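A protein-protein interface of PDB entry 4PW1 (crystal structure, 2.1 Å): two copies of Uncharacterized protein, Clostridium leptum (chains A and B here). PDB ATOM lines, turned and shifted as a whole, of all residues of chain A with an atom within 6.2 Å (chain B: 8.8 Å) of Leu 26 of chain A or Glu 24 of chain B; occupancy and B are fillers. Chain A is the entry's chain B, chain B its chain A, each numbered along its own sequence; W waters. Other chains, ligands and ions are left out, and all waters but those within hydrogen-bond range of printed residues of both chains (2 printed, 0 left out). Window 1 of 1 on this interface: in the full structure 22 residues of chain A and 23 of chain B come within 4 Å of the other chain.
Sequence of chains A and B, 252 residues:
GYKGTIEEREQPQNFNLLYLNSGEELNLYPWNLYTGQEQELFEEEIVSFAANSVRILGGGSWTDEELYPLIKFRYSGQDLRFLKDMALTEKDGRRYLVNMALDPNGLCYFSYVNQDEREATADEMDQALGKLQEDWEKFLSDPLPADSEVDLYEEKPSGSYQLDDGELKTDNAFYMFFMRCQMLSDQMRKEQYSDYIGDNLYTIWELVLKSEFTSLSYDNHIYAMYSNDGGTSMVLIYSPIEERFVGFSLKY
The side-chain hydroxyl of Ser 233 of chain A sits at hydrogen-bond distance from the side-chain hydroxyl of Ser 22 of chain B, at 2.9 Å. The backbone carbonyl oxygen of Glu 25 of chain A is in hydrogen-bond range of the backbone NH of Asn 27 of chain B, at 2.7 Å. The backbone NH (N) of Gly 23 of chain B lies within hydrogen-bond range of the side-chain hydroxyl (OG) of Ser 233 of chain A (2.9 Å). The backbone carbonyl oxygen (O) of Gly 23 of chain B sits at hydrogen-bond distance from the backbone NH (N) of Tyr 29 of chain A. The side-chain amino group (NZ) of Lys 251 of chain A lies within hydrogen-bond range of the backbone carbonyl oxygen (O) of Ser 22 of chain B (3.3 Å). OD1 of Asn 21 of chain B lies within hydrogen-bond range of OG of Ser 233 of chain A (3.4 Å). ND2 of Asn 27 of chain A lies close to ND2 of Asn 27 of chain B (3.2 Å). SD of Met 225 of chain A lies close to OE2 of Glu 24 of chain B, 3.1 Å away. O of Glu 25 of chain B is in hydrogen-bond range of N of Asn 27 of chain A (2.8 Å).
The backbone NH of Leu 26 of chain A lies within hydrogen-bond range of the side-chain hydroxyl of Tyr 218 of chain A (3.1 Å). The backbone NH (N) of Asn 21 of chain B is in hydrogen-bond range of the side-chain carboxylate (OE1) of Glu 24 of chain B (2.8 Å). The side-chain amide nitrogen (ND2) of Asn 27 of chain A sits at hydrogen-bond distance from the side-chain carboxylate (OE1) of Glu 25 of chain A, 3.3 Å away. The backbone carbonyl oxygen of Leu 18 of chain B is in hydrogen-bond range of the backbone NH of Ser 217 of chain B, at 2.7 Å. The side-chain carboxylate of Glu 25 of chain B lies within hydrogen-bond range of the side-chain amide nitrogen of Asn 27 of chain B (3.3 Å). N of Tyr 223 of chain A is in hydrogen-bond range of O of Leu 216 of chain A, at 2.8 Å.
Among the printed residues, merely in contact across the chains: Met 225 of chain A with Tyr 19 of chain B (3.2 Å), Leu 28 of chain A with Gly 23 of chain B (3.3 Å), Leu 26 of chain A with Glu 25 of chain B (3.4 Å), Glu 25 of chain A with Leu 26 of chain B (3.4 Å), Glu 25 of chain A with Glu 25 of chain B (3.5 Å), Glu 25 of chain A with Asn 32 of chain B (3.5 Å), Met 225 of chain A with Asn 21 of chain B (3.6 Å), Leu 28 of chain A with Glu 24 of chain B (3.6 Å), Leu 216 of chain A with Leu 20 of chain B (3.7 Å), Leu 20 of chain A with Leu 216 of chain B (3.7 Å), Glu 24 of chain A with Leu 28 of chain B (3.7 Å), Asn 27 of chain A with Glu 24 of chain B (3.7 Å), Val 235 of chain A with Glu 24 of chain B (3.8 Å), Glu 24 of chain A with Asn 27 of chain B (3.8 Å), Leu 216 of chain A with Leu 18 of chain B (3.8 Å), Asn 27 of chain A with Gly 23 of chain B (3.9 Å), Glu 24 of chain A with Leu 26 of chain B (3.9 Å), Leu 26 of chain A with Glu 24 of chain B (3.9 Å) and Lys 251 of chain A with Gly 23 of chain B (3.9 Å).
Leu 26 of chain A touches just these residues of chain B: Glu 24 (3.9 Å) and Glu 25 (3.4 Å). Of the printed residues of chain A, Leu 28 of chain B touches Glu 24. Printed residues of chain A within 4 Å of Leu 20 of chain B: Leu 216. Of the printed residues of chain A, Leu 216 of chain B touches Leu 20. Printed residues of chain B within 4 Å of Ser 233 of chain A: Asn 21, Ser 22 and Gly 23. Tyr 223 of chain A touches none of the printed residues of chain B. The nearest residue of chain A that does not touch Glu 24 of chain B is Leu 216 of chain A (4.3 Å). The nearest printed residue of chain A that does not touch Leu 20 of chain B is Met 225 of chain A (4.1 Å).
Hydrophobic or aromatic side chains of chain B that line the printed part of chain A: Leu 18, Leu 20, Leu 26, Leu 28 and Leu 216. Along chain B the printed residues that touch a printed residue of chain A span positions 18 to 216. Hydrophobic or aromatic side chains of chain A within 4 Å of the printed part of chain B: Leu 20, Leu 26, Leu 28, Tyr 29, Leu 216, Met 225 and Val 235. Among the printed residues, no Asp or Glu carboxylate lies within 4 Å of a Lys or Arg side-chain nitrogen of the other chain.
Leu 20 of chain A touches Leu 216 of chain B, and with the chains exchanged Leu 216 of chain A touches Leu 20 of chain B. Glu 24 of chain A touches Leu 28 of chain B, and with the chains exchanged Leu 28 of chain A touches Glu 24 of chain B. Glu 25 of chain A touches Asn 27 of chain B, and with the chains exchanged Asn 27 of chain A touches Glu 25 of chain B. Asn 27 of chain A touches its own counterpart, Asn 27 of chain B. 8 positions are printed for both chains.
Water W2 lies within hydrogen-bond range of OD1 of Asn 21 of chain B (2.5 Å), OG of Ser 233 of chain A (2.8 Å) and N of Gly 23 of chain B (3.5 Å). Water W1 bridges the backbone carbonyl oxygen (O) of Asn 32 of chain B (2.9 Å) and the side-chain carboxylate (OE2) of Glu 25 of chain A (3.0 Å).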
ATOM      1  N   LEU A  20      -8.000  26.638   5.658  1.00  0.00           N
ATOM      2  CA  LEU A  20      -9.169  26.564   4.761  1.00  0.00           C
ATOM      3  C   LEU A  20     -10.515  26.500   5.526  1.00  0.00           C
ATOM      4  O   LEU A  20     -10.548  25.991   6.590  1.00  0.00           O
ATOM      5  CB  LEU A  20      -9.045  25.383   3.812  1.00  0.00           C
ATOM      6  CG  LEU A  20      -7.862  25.439   2.888  1.00  0.00           C
ATOM      7  CD1 LEU A  20      -7.993  24.320   1.860  1.00  0.00           C
ATOM      8  CD2 LEU A  20      -7.732  26.759   2.184  1.00  0.00           C
ATOM      9  N   GLU A  24     -14.717  24.717   1.554  1.00  0.00           N
ATOM     10  CA  GLU A  24     -13.608  24.422   0.715  1.00  0.00           C
ATOM     11  C   GLU A  24     -13.260  22.930   0.901  1.00  0.00           C
ATOM     12  O   GLU A  24     -12.953  22.478   1.993  1.00  0.00           O
ATOM     13  CB  GLU A  24     -12.417  25.375   1.045  1.00  0.00           C
ATOM     14  CG  GLU A  24     -12.613  26.856   0.600  1.00  0.00           C
ATOM     15  CD  GLU A  24     -11.522  27.856   1.093  1.00  0.00           C
ATOM     16  OE1 GLU A  24     -11.128  27.787   2.283  1.00  0.00           O
ATOM     17  OE2 GLU A  24     -11.058  28.745   0.312  1.00  0.00           O
ATOM     18  N   GLU A  25     -13.333  22.184  -0.190  1.00  0.00           N
ATOM     19  CA  GLU A  25     -12.801  20.851  -0.276  1.00  0.00           C
ATOM     20  C   GLU A  25     -11.478  20.922  -1.071  1.00  0.00           C
ATOM     21  O   GLU A  25     -11.427  21.431  -2.204  1.00  0.00           O
ATOM     22  CB  GLU A  25     -13.788  19.909  -0.961  1.00  0.00           C
ATOM     23  CG  GLU A  25     -13.237  18.500  -1.210  1.00  0.00           C
ATOM     24  CD  GLU A  25     -14.165  17.620  -2.044  1.00  0.00           C
ATOM     25  OE1 GLU A  25     -14.364  17.843  -3.270  1.00  0.00           O
ATOM     26  OE2 GLU A  25     -14.725  16.694  -1.460  1.00  0.00           O
ATOM     27  N   LEU A  26     -10.424  20.419  -0.460  1.00  0.00           N
ATOM     28  CA  LEU A  26      -9.139  20.329  -1.083  1.00  0.00           C
ATOM     29  C   LEU A  26      -8.861  18.870  -1.405  1.00  0.00           C
ATOM     30  O   LEU A  26      -8.767  18.067  -0.502  1.00  0.00           O
ATOM     31  CB  LEU A  26      -8.073  20.883  -0.134  1.00  0.00           C
ATOM     32  CG  LEU A  26      -6.623  20.901  -0.618  1.00  0.00           C
ATOM     33  CD1 LEU A  26      -6.486  21.775  -1.854  1.00  0.00           C
ATOM     34  CD2 LEU A  26      -5.725  21.440   0.486  1.00  0.00           C
ATOM     35  N   ASN A  27      -8.755  18.535  -2.685  1.00  0.00           N
ATOM     36  CA  ASN A  27      -8.390  17.203  -3.094  1.00  0.00           C
ATOM     37  C   ASN A  27      -6.959  17.209  -3.606  1.00  0.00           C
ATOM     38  O   ASN A  27      -6.637  17.956  -4.526  1.00  0.00           O
ATOM     39  CB  ASN A  27      -9.248  16.721  -4.255  1.00  0.00           C
ATOM     40  CG  ASN A  27     -10.694  16.515  -3.876  1.00  0.00           C
ATOM     41  OD1 ASN A  27     -11.012  16.070  -2.793  1.00  0.00           O
ATOM     42  ND2 ASN A  27     -11.579  16.885  -4.764  1.00  0.00           N
ATOM     43  N   LEU A  28      -6.131  16.361  -3.044  1.00  0.00           N
ATOM     44  CA  LEU A  28      -4.765  16.186  -3.560  1.00  0.00           C
ATOM     45  C   LEU A  28      -4.717  15.139  -4.660  1.00  0.00           C
ATOM     46  O   LEU A  28      -5.517  14.189  -4.657  1.00  0.00           O
ATOM     47  CB  LEU A  28      -3.848  15.784  -2.412  1.00  0.00           C
ATOM     48  CG  LEU A  28      -3.828  16.753  -1.231  1.00  0.00           C
ATOM     49  CD1 LEU A  28      -2.829  16.249  -0.195  1.00  0.00           C
ATOM     50  CD2 LEU A  28      -3.497  18.161  -1.686  1.00  0.00           C
ATOM     51  N   TYR A  29      -3.838  15.353  -5.615  1.00  0.00           N
ATOM     52  CA  TYR A  29      -3.638  14.438  -6.724  1.00  0.00           C
ATOM     53  C   TYR A  29      -3.410  13.032  -6.137  1.00  0.00           C
ATOM     54  O   TYR A  29      -2.685  12.885  -5.148  1.00  0.00           O
ATOM     55  CB  TYR A  29      -2.480  14.901  -7.622  1.00  0.00           C
ATOM     56  CG  TYR A  29      -2.151  13.881  -8.709  1.00  0.00           C
ATOM     57  CD1 TYR A  29      -2.831  13.891  -9.944  1.00  0.00           C
ATOM     58  CD2 TYR A  29      -1.205  12.877  -8.465  1.00  0.00           C
ATOM     59  CE1 TYR A  29      -2.553  12.960 -10.924  1.00  0.00           C
ATOM     60  CE2 TYR A  29      -0.917  11.937  -9.440  1.00  0.00           C
ATOM     61  CZ  TYR A  29      -1.582  11.977 -10.649  1.00  0.00           C
ATOM     62  OH  TYR A  29      -1.328  11.004 -11.549  1.00  0.00           O
ATOM     63  N   LEU A 216      -0.384  25.383   4.248  1.00  0.00           N
ATOM     64  CA  LEU A 216      -1.717  25.773   4.732  1.00  0.00           C
ATOM     65  C   LEU A 216      -2.176  24.701   5.717  1.00  0.00           C
ATOM     66  O   LEU A 216      -1.575  23.612   5.801  1.00  0.00           O
ATOM     67  CB  LEU A 216      -2.696  25.909   3.558  1.00  0.00           C
ATOM     68  CG  LEU A 216      -2.941  24.683   2.682  1.00  0.00           C
ATOM     69  CD1 LEU A 216      -3.759  23.598   3.383  1.00  0.00           C
ATOM     70  CD2 LEU A 216      -3.641  25.108   1.381  1.00  0.00           C
ATOM     71  N   TYR A 218      -5.364  22.374   6.864  1.00  0.00           N
ATOM     72  CA  TYR A 218      -6.611  21.784   6.427  1.00  0.00           C
ATOM     73  C   TYR A 218      -6.847  20.514   7.228  1.00  0.00           C
ATOM     74  O   TYR A 218      -5.960  19.670   7.335  1.00  0.00           O
ATOM     75  CB  TYR A 218      -6.467  21.394   4.960  1.00  0.00           C
ATOM     76  CG  TYR A 218      -7.699  20.794   4.315  1.00  0.00           C
ATOM     77  CD1 TYR A 218      -8.872  21.560   4.100  1.00  0.00           C
ATOM     78  CD2 TYR A 218      -7.683  19.478   3.857  1.00  0.00           C
ATOM     79  CE1 TYR A 218      -9.988  21.018   3.438  1.00  0.00           C
ATOM     80  CE2 TYR A 218      -8.789  18.928   3.233  1.00  0.00           C
ATOM     81  CZ  TYR A 218      -9.931  19.708   3.018  1.00  0.00           C
ATOM     82  OH  TYR A 218     -10.993  19.180   2.353  1.00  0.00           O
ATOM     83  N   TYR A 223      -0.387  21.110   5.503  1.00  0.00           N
ATOM     84  CA  TYR A 223       0.021  20.667   4.148  1.00  0.00           C
ATOM     85  C   TYR A 223       1.246  21.464   3.735  1.00  0.00           C
ATOM     86  O   TYR A 223       1.183  22.666   3.541  1.00  0.00           O
ATOM     87  CB  TYR A 223      -1.115  20.870   3.143  1.00  0.00           C
ATOM     88  CG  TYR A 223      -2.218  19.837   3.221  1.00  0.00           C
ATOM     89  CD1 TYR A 223      -2.491  19.153   4.367  1.00  0.00           C
ATOM     90  CD2 TYR A 223      -3.050  19.607   2.138  1.00  0.00           C
ATOM     91  CE1 TYR A 223      -3.512  18.218   4.434  1.00  0.00           C
ATOM     92  CE2 TYR A 223      -4.071  18.682   2.201  1.00  0.00           C
ATOM     93  CZ  TYR A 223      -4.270  17.974   3.350  1.00  0.00           C
ATOM     94  OH  TYR A 223      -5.294  17.099   3.429  1.00  0.00           O
ATOM     95  N   MET A 225       3.927  22.284   1.039  1.00  0.00           N
ATOM     96  CA  MET A 225       3.768  22.247  -0.400  1.00  0.00           C
ATOM     97  C   MET A 225       5.053  22.622  -1.062  1.00  0.00           C
ATOM     98  O   MET A 225       5.752  23.589  -0.674  1.00  0.00           O
ATOM     99  CB  MET A 225       2.645  23.213  -0.827  1.00  0.00           C
ATOM    100  CG  MET A 225       1.310  22.735  -0.246  1.00  0.00           C
ATOM    101  SD  MET A 225       0.095  24.315  -0.088  1.00  0.00           S
ATOM    102  CE  MET A 225       0.668  25.346  -1.607  1.00  0.00           C
ATOM    103  N   SER A 233       4.661  18.691  -8.598  1.00  0.00           N
ATOM    104  CA  SER A 233       4.409  19.247  -7.296  1.00  0.00           C
ATOM    105  C   SER A 233       4.099  18.163  -6.283  1.00  0.00           C
ATOM    106  O   SER A 233       3.706  17.037  -6.623  1.00  0.00           O
ATOM    107  CB  SER A 233       3.281  20.309  -7.386  1.00  0.00           C
ATOM    108  OG  SER A 233       2.044  19.694  -7.606  1.00  0.00           O
ATOM    109  N   VAL A 235       2.714  17.515  -1.970  1.00  0.00           N
ATOM    110  CA  VAL A 235       2.290  17.928  -0.661  1.00  0.00           C
ATOM    111  C   VAL A 235       2.675  16.862   0.327  1.00  0.00           C
ATOM    112  O   VAL A 235       2.464  15.673   0.090  1.00  0.00           O
ATOM    113  CB  VAL A 235       0.765  18.129  -0.622  1.00  0.00           C
ATOM    114  CG1 VAL A 235       0.331  18.507   0.765  1.00  0.00           C
ATOM    115  CG2 VAL A 235       0.353  19.169  -1.612  1.00  0.00           C
ATOM    116  N   LYS A 251       2.619  14.619  -7.736  1.00  0.00           N
ATOM    117  CA  LYS A 251       2.137  14.707  -9.105  1.00  0.00           C
ATOM    118  C   LYS A 251       3.272  15.160 -10.027  1.00  0.00           C
ATOM    119  O   LYS A 251       3.737  16.291  -9.921  1.00  0.00           O
ATOM    120  CB  LYS A 251       1.009  15.722  -9.210  1.00  0.00           C
ATOM    121  CG  LYS A 251       0.475  15.856 -10.621  1.00  0.00           C
ATOM    122  CD  LYS A 251      -0.601  16.938 -10.685  1.00  0.00           C
ATOM    123  CE  LYS A 251      -1.155  17.031 -12.075  1.00  0.00           C
ATOM    124  NZ  LYS A 251      -2.486  17.650 -11.983  1.00  0.00           N
ATOM    125  N   LEU B  18      -0.443  33.025  -0.626  1.00  0.00           N
ATOM    126  CA  LEU B  18      -0.274  31.608  -0.892  1.00  0.00           C
ATOM    127  C   LEU B  18      -0.865  31.163  -2.268  1.00  0.00           C
ATOM    128  O   LEU B  18      -2.057  31.362  -2.539  1.00  0.00           O
ATOM    129  CB  LEU B  18      -0.957  30.826   0.233  1.00  0.00           C
ATOM    130  CG  LEU B  18      -0.815  29.317   0.102  1.00  0.00           C
ATOM    131  CD1 LEU B  18       0.625  28.887   0.390  1.00  0.00           C
ATOM    132  CD2 LEU B  18      -1.800  28.639   1.033  1.00  0.00           C
ATOM    133  N   TYR B  19      -0.057  30.530  -3.113  1.00  0.00           N
ATOM    134  CA  TYR B  19      -0.564  29.919  -4.354  1.00  0.00           C
ATOM    135  C   TYR B  19      -0.755  28.438  -4.181  1.00  0.00           C
ATOM    136  O   TYR B  19       0.131  27.777  -3.653  1.00  0.00           O
ATOM    137  CB  TYR B  19       0.440  30.099  -5.480  1.00  0.00           C
ATOM    138  CG  TYR B  19       0.576  31.507  -5.939  1.00  0.00           C
ATOM    139  CD1 TYR B  19       1.249  32.450  -5.169  1.00  0.00           C
ATOM    140  CD2 TYR B  19      -0.006  31.918  -7.149  1.00  0.00           C
ATOM    141  CE1 TYR B  19       1.349  33.768  -5.579  1.00  0.00           C
ATOM    142  CE2 TYR B  19       0.107  33.230  -7.578  1.00  0.00           C
ATOM    143  CZ  TYR B  19       0.787  34.143  -6.783  1.00  0.00           C
ATOM    144  OH  TYR B  19       0.916  35.421  -7.209  1.00  0.00           O
ATOM    145  N   LEU B  20      -1.878  27.881  -4.596  1.00  0.00           N
ATOM    146  CA  LEU B  20      -2.004  26.424  -4.589  1.00  0.00           C
ATOM    147  C   LEU B  20      -1.211  25.828  -5.751  1.00  0.00           C
ATOM    148  O   LEU B  20      -1.087  26.460  -6.768  1.00  0.00           O
ATOM    149  CB  LEU B  20      -3.472  25.996  -4.660  1.00  0.00           C
ATOM    150  CG  LEU B  20      -4.304  26.384  -3.458  1.00  0.00           C
ATOM    151  CD1 LEU B  20      -5.673  25.716  -3.544  1.00  0.00           C
ATOM    152  CD2 LEU B  20      -3.660  26.029  -2.165  1.00  0.00           C
ATOM    153  N   ASN B  21      -0.672  24.623  -5.612  1.00  0.00           N
ATOM    154  CA  ASN B  21       0.187  24.063  -6.672  1.00  0.00           C
ATOM    155  C   ASN B  21      -0.600  23.137  -7.582  1.00  0.00           C
ATOM    156  O   ASN B  21      -1.845  22.985  -7.395  1.00  0.00           O
ATOM    157  CB  ASN B  21       1.508  23.462  -6.093  1.00  0.00           C
ATOM    158  CG  ASN B  21       1.293  22.254  -5.173  1.00  0.00           C
ATOM    159  OD1 ASN B  21       0.337  21.485  -5.334  1.00  0.00           O
ATOM    160  ND2 ASN B  21       2.218  22.059  -4.236  1.00  0.00           N
ATOM    161  N   SER B  22       0.066  22.536  -8.576  1.00  0.00           N
ATOM    162  CA  SER B  22      -0.660  21.772  -9.612  1.00  0.00           C
ATOM    163  C   SER B  22      -1.296  20.485  -9.052  1.00  0.00           C
ATOM    164  O   SER B  22      -2.224  19.957  -9.628  1.00  0.00           O
ATOM    165  CB  SER B  22       0.287  21.415 -10.761  1.00  0.00           C
ATOM    166  OG  SER B  22       1.342  20.610 -10.273  1.00  0.00           O
ATOM    167  N   GLY B  23      -0.801  19.993  -7.924  1.00  0.00           N
ATOM    168  CA  GLY B  23      -1.363  18.780  -7.278  1.00  0.00           C
ATOM    169  C   GLY B  23      -2.550  18.999  -6.350  1.00  0.00           C
ATOM    170  O   GLY B  23      -2.932  18.094  -5.596  1.00  0.00           O
ATOM    171  N   GLU B  24      -3.116  20.200  -6.394  1.00  0.00           N
ATOM    172  CA  GLU B  24      -4.156  20.587  -5.467  1.00  0.00           C
ATOM    173  C   GLU B  24      -5.372  21.049  -6.275  1.00  0.00           C
ATOM    174  O   GLU B  24      -5.291  21.952  -7.085  1.00  0.00           O
ATOM    175  CB  GLU B  24      -3.639  21.674  -4.504  1.00  0.00           C
ATOM    176  CG  GLU B  24      -2.612  21.212  -3.444  1.00  0.00           C
ATOM    177  CD  GLU B  24      -1.974  22.358  -2.619  1.00  0.00           C
ATOM    178  OE1 GLU B  24      -1.570  23.381  -3.240  1.00  0.00           O
ATOM    179  OE2 GLU B  24      -1.835  22.247  -1.347  1.00  0.00           O
ATOM    180  N   GLU B  25      -6.498  20.384  -6.070  1.00  0.00           N
ATOM    181  CA  GLU B  25      -7.783  20.803  -6.596  1.00  0.00           C
ATOM    182  C   GLU B  25      -8.610  21.352  -5.448  1.00  0.00           C
ATOM    183  O   GLU B  25      -8.810  20.688  -4.416  1.00  0.00           O
ATOM    184  CB  GLU B  25      -8.515  19.647  -7.292  1.00  0.00           C
ATOM    185  CG  GLU B  25      -9.942  19.981  -7.724  1.00  0.00           C
ATOM    186  CD  GLU B  25     -10.727  18.783  -8.230  1.00  0.00           C
ATOM    187  OE1 GLU B  25     -11.111  17.885  -7.411  1.00  0.00           O
ATOM    188  OE2 GLU B  25     -10.915  18.710  -9.470  1.00  0.00           O
ATOM    189  N   LEU B  26      -9.105  22.569  -5.638  1.00  0.00           N
ATOM    190  CA  LEU B  26      -9.949  23.218  -4.659  1.00  0.00           C
ATOM    191  C   LEU B  26     -11.357  23.255  -5.197  1.00  0.00           C
ATOM    192  O   LEU B  26     -11.596  23.881  -6.215  1.00  0.00           O
ATOM    193  CB  LEU B  26      -9.411  24.615  -4.406  1.00  0.00           C
ATOM    194  CG  LEU B  26     -10.118  25.470  -3.358  1.00  0.00           C
ATOM    195  CD1 LEU B  26     -10.093  24.814  -1.995  1.00  0.00           C
ATOM    196  CD2 LEU B  26      -9.426  26.821  -3.284  1.00  0.00           C
ATOM    197  N   ASN B  27     -12.275  22.523  -4.574  1.00  0.00           N
ATOM    198  CA  ASN B  27     -13.672  22.594  -4.954  1.00  0.00           C
ATOM    199  C   ASN B  27     -14.430  23.417  -3.925  1.00  0.00           C
ATOM    200  O   ASN B  27     -14.460  23.082  -2.754  1.00  0.00           O
ATOM    201  CB  ASN B  27     -14.331  21.221  -4.965  1.00  0.00           C
ATOM    202  CG  ASN B  27     -13.801  20.326  -6.037  1.00  0.00           C
ATOM    203  OD1 ASN B  27     -13.492  20.752  -7.139  1.00  0.00           O
ATOM    204  ND2 ASN B  27     -13.659  19.074  -5.706  1.00  0.00           N
ATOM    205  N   LEU B  28     -15.102  24.453  -4.368  1.00  0.00           N
ATOM    206  CA  LEU B  28     -15.942  25.232  -3.489  1.00  0.00           C
ATOM    207  C   LEU B  28     -17.343  24.626  -3.411  1.00  0.00           C
ATOM    208  O   LEU B  28     -17.860  24.054  -4.394  1.00  0.00           O
ATOM    209  CB  LEU B  28     -16.008  26.681  -4.007  1.00  0.00           C
ATOM    210  CG  LEU B  28     -14.656  27.403  -4.132  1.00  0.00           C
ATOM    211  CD1 LEU B  28     -14.849  28.828  -4.606  1.00  0.00           C
ATOM    212  CD2 LEU B  28     -13.902  27.362  -2.821  1.00  0.00           C
ATOM    213  N   ASN B  32     -18.284  20.056  -4.289  1.00  0.00           N
ATOM    214  CA  ASN B  32     -17.822  18.866  -3.589  1.00  0.00           C
ATOM    215  C   ASN B  32     -18.908  17.789  -3.549  1.00  0.00           C
ATOM    216  O   ASN B  32     -18.603  16.630  -3.325  1.00  0.00           O
ATOM    217  CB  ASN B  32     -17.406  19.205  -2.159  1.00  0.00           C
ATOM    218  CG  ASN B  32     -18.492  19.939  -1.405  1.00  0.00           C
ATOM    219  OD1 ASN B  32     -19.031  20.945  -1.882  1.00  0.00           O
ATOM    220  ND2 ASN B  32     -18.858  19.426  -0.256  1.00  0.00           N
ATOM    221  N   LEU B 216      -6.130  33.205  -0.723  1.00  0.00           N
ATOM    222  CA  LEU B 216      -5.149  32.387  -1.431  1.00  0.00           C
ATOM    223  C   LEU B 216      -5.369  32.609  -2.910  1.00  0.00           C
ATOM    224  O   LEU B 216      -6.393  33.204  -3.333  1.00  0.00           O
ATOM    225  CB  LEU B 216      -5.316  30.903  -1.082  1.00  0.00           C
ATOM    226  CG  LEU B 216      -6.632  30.205  -1.383  1.00  0.00           C
ATOM    227  CD1 LEU B 216      -6.878  29.999  -2.880  1.00  0.00           C
ATOM    228  CD2 LEU B 216      -6.718  28.874  -0.640  1.00  0.00           C
ATOM    229  N   SER B 217      -4.396  32.203  -3.704  1.00  0.00           N
ATOM    230  CA  SER B 217      -4.470  32.314  -5.161  1.00  0.00           C
ATOM    231  C   SER B 217      -4.587  30.930  -5.766  1.00  0.00           C
ATOM    232  O   SER B 217      -3.867  29.963  -5.384  1.00  0.00           O
ATOM    233  CB  SER B 217      -3.254  33.039  -5.726  1.00  0.00           C
ATOM    234  OG  SER B 217      -3.403  33.167  -7.136  1.00  0.00           O
ATOM    235  N   TYR B 218      -5.548  30.818  -6.655  1.00  0.00           N
ATOM    236  CA  TYR B 218      -5.847  29.566  -7.307  1.00  0.00           C
ATOM    237  C   TYR B 218      -6.386  29.880  -8.685  1.00  0.00           C
ATOM    238  O   TYR B 218      -7.277  30.723  -8.829  1.00  0.00           O
ATOM    239  CB  TYR B 218      -6.931  28.834  -6.528  1.00  0.00           C
ATOM    240  CG  TYR B 218      -7.350  27.512  -7.084  1.00  0.00           C
ATOM    241  CD1 TYR B 218      -6.478  26.410  -7.070  1.00  0.00           C
ATOM    242  CD2 TYR B 218      -8.624  27.340  -7.624  1.00  0.00           C
ATOM    243  CE1 TYR B 218      -6.878  25.180  -7.578  1.00  0.00           C
ATOM    244  CE2 TYR B 218      -9.024  26.129  -8.118  1.00  0.00           C
ATOM    245  CZ  TYR B 218      -8.162  25.058  -8.085  1.00  0.00           C
ATOM    246  OH  TYR B 218      -8.664  23.882  -8.566  1.00  0.00           O
ATOM    247  N   ASP B 219      -5.816  29.239  -9.672  1.00  0.00           N
ATOM    248  CA  ASP B 219      -6.332  29.290 -11.026  1.00  0.00           C
ATOM    249  C   ASP B 219      -6.458  30.739 -11.586  1.00  0.00           C
ATOM    250  O   ASP B 219      -7.488  31.108 -12.176  1.00  0.00           O
ATOM    251  CB  ASP B 219      -7.667  28.569 -11.033  1.00  0.00           C
ATOM    252  CG  ASP B 219      -8.133  28.246 -12.412  1.00  0.00           C
ATOM    253  OD1 ASP B 219      -7.264  28.054 -13.293  1.00  0.00           O
ATOM    254  OD2 ASP B 219      -9.358  28.254 -12.616  1.00  0.00           O
HETATM  255  O   HOH W   1     -16.101  15.276  -3.672  1.00  0.00           O
HETATM  256  O   HOH W   2       1.026  19.115  -5.107  1.00  0.00           O
